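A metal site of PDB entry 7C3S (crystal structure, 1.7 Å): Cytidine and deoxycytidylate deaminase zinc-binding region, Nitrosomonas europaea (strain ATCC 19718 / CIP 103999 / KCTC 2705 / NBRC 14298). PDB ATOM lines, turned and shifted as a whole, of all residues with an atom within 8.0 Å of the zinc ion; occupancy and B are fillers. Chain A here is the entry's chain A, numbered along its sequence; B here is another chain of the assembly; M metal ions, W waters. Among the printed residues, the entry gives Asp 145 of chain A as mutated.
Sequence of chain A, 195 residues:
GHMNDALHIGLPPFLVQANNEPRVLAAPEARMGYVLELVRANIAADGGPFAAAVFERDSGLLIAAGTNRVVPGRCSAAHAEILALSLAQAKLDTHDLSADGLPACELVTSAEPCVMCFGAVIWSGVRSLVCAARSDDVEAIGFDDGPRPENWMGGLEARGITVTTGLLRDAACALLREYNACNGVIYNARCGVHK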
ATOM      1  N   PHE A  50      36.615 -22.998  30.319  1.00  0.00           N
ATOM      2  CA  PHE A  50      35.791 -24.142  30.766  1.00  0.00           C
ATOM      3  C   PHE A  50      36.603 -25.419  30.709  1.00  0.00           C
ATOM      4  O   PHE A  50      37.291 -25.691  29.741  1.00  0.00           O
ATOM      5  CB  PHE A  50      34.508 -24.295  29.962  1.00  0.00           C
ATOM      6  CG  PHE A  50      33.635 -23.070  29.943  1.00  0.00           C
ATOM      7  CD1 PHE A  50      32.709 -22.856  30.931  1.00  0.00           C
ATOM      8  CD2 PHE A  50      33.816 -22.119  28.961  1.00  0.00           C
ATOM      9  CE1 PHE A  50      31.963 -21.679  30.946  1.00  0.00           C
ATOM     10  CE2 PHE A  50      33.062 -20.963  28.967  1.00  0.00           C
ATOM     11  CZ  PHE A  50      32.152 -20.735  29.964  1.00  0.00           C
ATOM     12  N   ASN A  68      37.118 -26.771  26.812  1.00  0.00           N
ATOM     13  CA  ASN A  68      36.447 -26.175  25.663  1.00  0.00           C
ATOM     14  C   ASN A  68      37.473 -25.974  24.544  1.00  0.00           C
ATOM     15  O   ASN A  68      38.426 -25.228  24.743  1.00  0.00           O
ATOM     16  CB  ASN A  68      35.843 -24.884  26.171  1.00  0.00           C
ATOM     17  CG  ASN A  68      35.098 -24.143  25.124  1.00  0.00           C
ATOM     18  OD1 ASN A  68      35.739 -23.775  24.133  1.00  0.00           O
ATOM     19  ND2 ASN A  68      33.808 -23.949  25.410  1.00  0.00           N
ATOM     20  N   VAL A  70      36.215 -25.338  21.276  1.00  0.00           N
ATOM     21  CA  VAL A  70      35.232 -24.967  20.226  1.00  0.00           C
ATOM     22  C   VAL A  70      35.899 -24.146  19.135  1.00  0.00           C
ATOM     23  O   VAL A  70      35.743 -24.477  17.973  1.00  0.00           O
ATOM     24  CB  VAL A  70      34.080 -24.190  20.849  1.00  0.00           C
ATOM     25  CG1 VAL A  70      33.183 -23.537  19.822  1.00  0.00           C
ATOM     26  CG2 VAL A  70      33.284 -25.104  21.761  1.00  0.00           C
ATOM     27  N   SER A  76      31.691 -26.843  17.313  1.00  0.00           N
ATOM     28  CA  SER A  76      30.800 -26.217  18.312  1.00  0.00           C
ATOM     29  C   SER A  76      30.429 -27.254  19.391  1.00  0.00           C
ATOM     30  O   SER A  76      30.068 -26.838  20.495  1.00  0.00           O
ATOM     31  CB  SER A  76      29.570 -25.597  17.703  1.00  0.00           C
ATOM     32  OG  SER A  76      28.833 -26.560  16.973  1.00  0.00           O
ATOM     33  N   ALA A  77      30.539 -28.552  19.116  1.00  0.00           N
ATOM     34  CA  ALA A  77      30.224 -29.601  20.123  1.00  0.00           C
ATOM     35  C   ALA A  77      31.371 -29.789  21.105  1.00  0.00           C
ATOM     36  O   ALA A  77      31.166 -30.557  22.079  1.00  0.00           O
ATOM     37  CB  ALA A  77      29.895 -30.898  19.438  1.00  0.00           C
ATOM     38  N   ALA A  78      32.551 -29.190  20.899  1.00  0.00           N
ATOM     39  CA  ALA A  78      33.773 -29.474  21.697  1.00  0.00           C
ATOM     40  C   ALA A  78      33.745 -28.696  23.011  1.00  0.00           C
ATOM     41  O   ALA A  78      34.749 -28.023  23.390  1.00  0.00           O
ATOM     42  CB  ALA A  78      35.016 -29.160  20.888  1.00  0.00           C
ATOM     43  N   HIS A  79      32.646 -28.803  23.738  1.00  0.00           N
ATOM     44  CA  HIS A  79      32.519 -28.312  25.136  1.00  0.00           C
ATOM     45  C   HIS A  79      33.310 -29.247  26.048  1.00  0.00           C
ATOM     46  O   HIS A  79      33.482 -30.430  25.719  1.00  0.00           O
ATOM     47  CB  HIS A  79      31.071 -28.233  25.581  1.00  0.00           C
ATOM     48  CG  HIS A  79      30.309 -27.126  24.952  1.00  0.00           C
ATOM     49  ND1 HIS A  79      29.152 -26.608  25.513  1.00  0.00           N
ATOM     50  CD2 HIS A  79      30.545 -26.428  23.810  1.00  0.00           C
ATOM     51  CE1 HIS A  79      28.682 -25.657  24.721  1.00  0.00           C
ATOM     52  NE2 HIS A  79      29.522 -25.511  23.680  1.00  0.00           N
ATOM     53  N   ALA A  80      33.841 -28.700  27.126  1.00  0.00           N
ATOM     54  CA  ALA A  80      34.642 -29.454  28.116  1.00  0.00           C
ATOM     55  C   ALA A  80      33.903 -30.761  28.516  1.00  0.00           C
ATOM     56  O   ALA A  80      34.519 -31.804  28.580  1.00  0.00           O
ATOM     57  CB  ALA A  80      34.884 -28.582  29.314  1.00  0.00           C
ATOM     58  N   GLU A  81      32.611 -30.676  28.772  1.00  0.00           N
ATOM     59  CA  GLU A  81      31.833 -31.836  29.289  1.00  0.00           C
ATOM     60  C   GLU A  81      31.781 -32.950  28.246  1.00  0.00           C
ATOM     61  O   GLU A  81      31.986 -34.143  28.555  1.00  0.00           O
ATOM     62  CB  GLU A  81      30.437 -31.379  29.686  1.00  0.00           C
ATOM     63  CG  GLU A  81      30.436 -30.258  30.708  1.00  0.00           C
ATOM     64  CD  GLU A  81      30.275 -28.882  30.080  1.00  0.00           C
ATOM     65  OE1 GLU A  81      31.131 -28.502  29.242  1.00  0.00           O
ATOM     66  OE2 GLU A  81      29.278 -28.178  30.466  1.00  0.00           O
ATOM     67  N   ILE A  82      31.510 -32.591  27.000  1.00  0.00           N
ATOM     68  CA  ILE A  82      31.476 -33.561  25.876  1.00  0.00           C
ATOM     69  C   ILE A  82      32.840 -34.228  25.753  1.00  0.00           C
ATOM     70  O   ILE A  82      32.874 -35.413  25.599  1.00  0.00           O
ATOM     71  CB  ILE A  82      31.074 -32.895  24.544  1.00  0.00           C
ATOM     72  CG1 ILE A  82      29.720 -32.201  24.605  1.00  0.00           C
ATOM     73  CG2 ILE A  82      31.139 -33.909  23.418  1.00  0.00           C
ATOM     74  CD1 ILE A  82      28.581 -33.056  24.942  1.00  0.00           C
ATOM     75  N   THR A 109      32.792 -30.329  36.795  1.00  0.00           N
ATOM     76  CA  THR A 109      32.773 -29.337  35.700  1.00  0.00           C
ATOM     77  C   THR A 109      32.921 -27.930  36.299  1.00  0.00           C
ATOM     78  O   THR A 109      32.303 -27.626  37.348  1.00  0.00           O
ATOM     79  CB  THR A 109      31.490 -29.517  34.858  1.00  0.00           C
ATOM     80  OG1 THR A 109      31.574 -28.607  33.766  1.00  0.00           O
ATOM     81  CG2 THR A 109      30.246 -29.285  35.666  1.00  0.00           C
ATOM     82  N   ALA A 111      31.675 -25.203  35.297  1.00  0.00           N
ATOM     83  CA  ALA A 111      30.430 -24.426  35.210  1.00  0.00           C
ATOM     84  C   ALA A 111      29.281 -25.404  34.969  1.00  0.00           C
ATOM     85  O   ALA A 111      29.513 -26.520  34.455  1.00  0.00           O
ATOM     86  CB  ALA A 111      30.480 -23.347  34.165  1.00  0.00           C
ATOM     87  N   GLU A 112      28.100 -24.995  35.380  1.00  0.00           N
ATOM     88  CA  GLU A 112      26.856 -25.732  35.121  1.00  0.00           C
ATOM     89  C   GLU A 112      26.730 -25.959  33.626  1.00  0.00           C
ATOM     90  O   GLU A 112      26.996 -25.064  32.819  1.00  0.00           O
ATOM     91  CB  GLU A 112      25.677 -24.961  35.672  1.00  0.00           C
ATOM     92  CG  GLU A 112      25.664 -25.014  37.193  1.00  0.00           C
ATOM     93  CD  GLU A 112      24.595 -24.162  37.852  1.00  0.00           C
ATOM     94  OE1 GLU A 112      23.836 -23.508  37.103  1.00  0.00           O
ATOM     95  OE2 GLU A 112      24.555 -24.181  39.091  1.00  0.00           O
ATOM     96  N   PRO A 113      26.260 -27.159  33.223  1.00  0.00           N
ATOM     97  CA  PRO A 113      26.232 -27.532  31.811  1.00  0.00           C
ATOM     98  C   PRO A 113      25.177 -26.781  31.008  1.00  0.00           C
ATOM     99  O   PRO A 113      24.102 -26.577  31.490  1.00  0.00           O
ATOM    100  CB  PRO A 113      25.912 -29.030  31.848  1.00  0.00           C
ATOM    101  CG  PRO A 113      25.108 -29.185  33.122  1.00  0.00           C
ATOM    102  CD  PRO A 113      25.794 -28.231  34.105  1.00  0.00           C
ATOM    103  N   CYS A 114      25.516 -26.416  29.757  1.00  0.00           N
ATOM    104  CA  CYS A 114      24.540 -25.883  28.812  1.00  0.00           C
ATOM    105  C   CYS A 114      23.514 -26.987  28.478  1.00  0.00           C
ATOM    106  O   CYS A 114      23.641 -28.149  28.888  1.00  0.00           O
ATOM    107  CB  CYS A 114      25.212 -25.388  27.555  1.00  0.00           C
ATOM    108  SG  CYS A 114      25.791 -26.691  26.443  1.00  0.00           S
ATOM    109  N   VAL A 115      22.498 -26.638  27.717  1.00  0.00           N
ATOM    110  CA  VAL A 115      21.439 -27.624  27.406  1.00  0.00           C
ATOM    111  C   VAL A 115      22.013 -28.817  26.635  1.00  0.00           C
ATOM    112  O   VAL A 115      21.572 -29.963  26.889  1.00  0.00           O
ATOM    113  CB  VAL A 115      20.263 -26.986  26.642  1.00  0.00           C
ATOM    114  CG1 VAL A 115      20.699 -26.366  25.342  1.00  0.00           C
ATOM    115  CG2 VAL A 115      19.163 -28.031  26.433  1.00  0.00           C
ATOM    116  N   MET A 116      22.948 -28.618  25.714  1.00  0.00           N
ATOM    117  CA  MET A 116      23.610 -29.732  24.972  1.00  0.00           C
ATOM    118  C   MET A 116      24.276 -30.666  25.996  1.00  0.00           C
ATOM    119  O   MET A 116      24.074 -31.901  25.977  1.00  0.00           O
ATOM    120  CB  MET A 116      24.670 -29.184  24.023  1.00  0.00           C
ATOM    121  CG  MET A 116      25.487 -30.279  23.299  1.00  0.00           C
ATOM    122  SD  MET A 116      26.633 -29.635  22.103  1.00  0.00           S
ATOM    123  CE  MET A 116      27.844 -28.898  23.198  1.00  0.00           C
ATOM    124  N   CYS A 117      25.128 -30.123  26.844  1.00  0.00           N
ATOM    125  CA  CYS A 117      25.910 -30.907  27.825  1.00  0.00           C
ATOM    126  C   CYS A 117      25.002 -31.566  28.881  1.00  0.00           C
ATOM    127  O   CYS A 117      25.354 -32.634  29.365  1.00  0.00           O
ATOM    128  CB  CYS A 117      27.026 -30.062  28.417  1.00  0.00           C
ATOM    129  SG  CYS A 117      28.244 -29.688  27.137  1.00  0.00           S
ATOM    130  N   PHE A 118      23.908 -30.924  29.262  1.00  0.00           N
ATOM    131  CA  PHE A 118      22.866 -31.505  30.138  1.00  0.00           C
ATOM    132  C   PHE A 118      22.369 -32.812  29.520  1.00  0.00           C
ATOM    133  O   PHE A 118      22.350 -33.880  30.190  1.00  0.00           O
ATOM    134  CB  PHE A 118      21.743 -30.495  30.290  1.00  0.00           C
ATOM    135  CG  PHE A 118      20.469 -31.067  30.852  1.00  0.00           C
ATOM    136  CD1 PHE A 118      20.361 -31.346  32.205  1.00  0.00           C
ATOM    137  CD2 PHE A 118      19.360 -31.209  30.044  1.00  0.00           C
ATOM    138  CE1 PHE A 118      19.166 -31.840  32.695  1.00  0.00           C
ATOM    139  CE2 PHE A 118      18.144 -31.629  30.561  1.00  0.00           C
ATOM    140  CZ  PHE A 118      18.073 -31.968  31.882  1.00  0.00           C
ATOM    141  N   ALA A 120      23.934 -34.575  27.210  1.00  0.00           N
ATOM    142  CA  ALA A 120      25.105 -35.481  27.194  1.00  0.00           C
ATOM    143  C   ALA A 120      25.318 -36.174  28.549  1.00  0.00           C
ATOM    144  O   ALA A 120      25.665 -37.382  28.582  1.00  0.00           O
ATOM    145  CB  ALA A 120      26.348 -34.742  26.758  1.00  0.00           C
ATOM    146  N   ASP A 144      26.516 -18.020  27.080  1.00  0.00           N
ATOM    147  CA  ASP A 144      25.118 -18.448  26.778  1.00  0.00           C
ATOM    148  C   ASP A 144      25.006 -19.967  26.965  1.00  0.00           C
ATOM    149  O   ASP A 144      25.581 -20.705  26.123  1.00  0.00           O
ATOM    150  CB  ASP A 144      24.728 -17.998  25.360  1.00  0.00           C
ATOM    151  CG  ASP A 144      23.305 -18.303  24.911  1.00  0.00           C
ATOM    152  OD1 ASP A 144      22.479 -18.697  25.762  1.00  0.00           O
ATOM    153  OD2 ASP A 144      23.034 -18.135  23.678  1.00  0.00           O
ATOM    154  N   ASP A 145      24.199 -20.406  27.948  1.00  0.00           N
ATOM    155  CA  ASP A 145      23.903 -21.832  28.289  1.00  0.00           C
ATOM    156  C   ASP A 145      22.686 -22.364  27.535  1.00  0.00           C
ATOM    157  O   ASP A 145      22.412 -23.642  27.575  1.00  0.00           O
ATOM    158  CB  ASP A 145      23.722 -21.984  29.792  1.00  0.00           C
ATOM    159  CG  ASP A 145      25.046 -21.871  30.537  1.00  0.00           C
ATOM    160  OD1 ASP A 145      26.112 -21.837  29.846  1.00  0.00           O
ATOM    161  OD2 ASP A 145      25.005 -21.796  31.790  1.00  0.00           O
ATOM    162  N   ARG A 148      17.868 -24.478  28.734  1.00  0.00           N
ATOM    163  CA  ARG A 148      17.805 -25.732  29.552  1.00  0.00           C
ATOM    164  C   ARG A 148      16.390 -25.912  30.042  1.00  0.00           C
ATOM    165  O   ARG A 148      15.747 -24.917  30.357  1.00  0.00           O
ATOM    166  CB  ARG A 148      18.667 -25.655  30.805  1.00  0.00           C
ATOM    167  CG  ARG A 148      20.056 -26.245  30.689  1.00  0.00           C
ATOM    168  CD  ARG A 148      20.789 -25.991  31.996  1.00  0.00           C
ATOM    169  NE  ARG A 148      20.844 -24.542  32.100  1.00  0.00           N
ATOM    170  CZ  ARG A 148      21.913 -23.782  32.252  1.00  0.00           C
ATOM    171  NH1 ARG A 148      23.122 -24.299  32.444  1.00  0.00           N
ATOM    172  NH2 ARG A 148      21.738 -22.472  32.257  1.00  0.00           N
ATOM    173  N   GLY B 119      20.509 -28.811  21.741  1.00  0.00           N
ATOM    174  CA  GLY B 119      21.579 -27.873  22.112  1.00  0.00           C
ATOM    175  C   GLY B 119      22.633 -27.757  21.023  1.00  0.00           C
ATOM    176  O   GLY B 119      23.079 -26.629  20.683  1.00  0.00           O
ATOM    177  N   TRP B 123      24.114 -24.353  18.986  1.00  0.00           N
ATOM    178  CA  TRP B 123      25.520 -23.872  18.973  1.00  0.00           C
ATOM    179  C   TRP B 123      26.115 -23.874  17.556  1.00  0.00           C
ATOM    180  O   TRP B 123      27.172 -23.223  17.323  1.00  0.00           O
ATOM    181  CB  TRP B 123      26.397 -24.636  19.970  1.00  0.00           C
ATOM    182  CG  TRP B 123      25.869 -24.599  21.376  1.00  0.00           C
ATOM    183  CD1 TRP B 123      25.804 -25.666  22.223  1.00  0.00           C
ATOM    184  CD2 TRP B 123      25.212 -23.519  22.066  1.00  0.00           C
ATOM    185  NE1 TRP B 123      25.259 -25.318  23.412  1.00  0.00           N
ATOM    186  CE2 TRP B 123      24.836 -24.013  23.335  1.00  0.00           C
ATOM    187  CE3 TRP B 123      24.875 -22.200  21.736  1.00  0.00           C
ATOM    188  CZ2 TRP B 123      24.188 -23.227  24.279  1.00  0.00           C
ATOM    189  CZ3 TRP B 123      24.259 -21.398  22.689  1.00  0.00           C
ATOM    190  CH2 TRP B 123      23.899 -21.917  23.935  1.00  0.00           C
HETATM  191 ZN    ZN M   1      27.936 -27.439  26.942  1.00  0.00          ZN
HETATM  192  O   HOH W   1      28.298 -26.563  28.724  1.00  0.00           O
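A ring nitrogen (NE2) of His 79 sits close to the backbone carbonyl oxygen of Ser 76 (3.5 Å).
The side-chain sulfur (SG) of Cys 117 sits close to the side-chain carboxylate (OE1) of Glu 81 (3.8 Å).
N of Met 116 sits close to SG of Cys 114.
SG of Cys 114 sits close to NE1 of Trp 123 of chain B.
Residues that only touch the zinc ion: Glu 81 (3.8 Å).
Of the 25 residues printed, 4 come within 4 Å of the zinc ion.
The zinc ion is bound by water W1 (2.0 Å), ND1 of His 79 (2.1 Å), SG of Cys 117 (2.3 Å) and SG of Cys 114 (2.3 Å).
The zinc ion has four donor atoms within binding distance.
Water W1 bridges the side-chain carboxylate of Glu 81 and the backbone NH of Cys 114.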
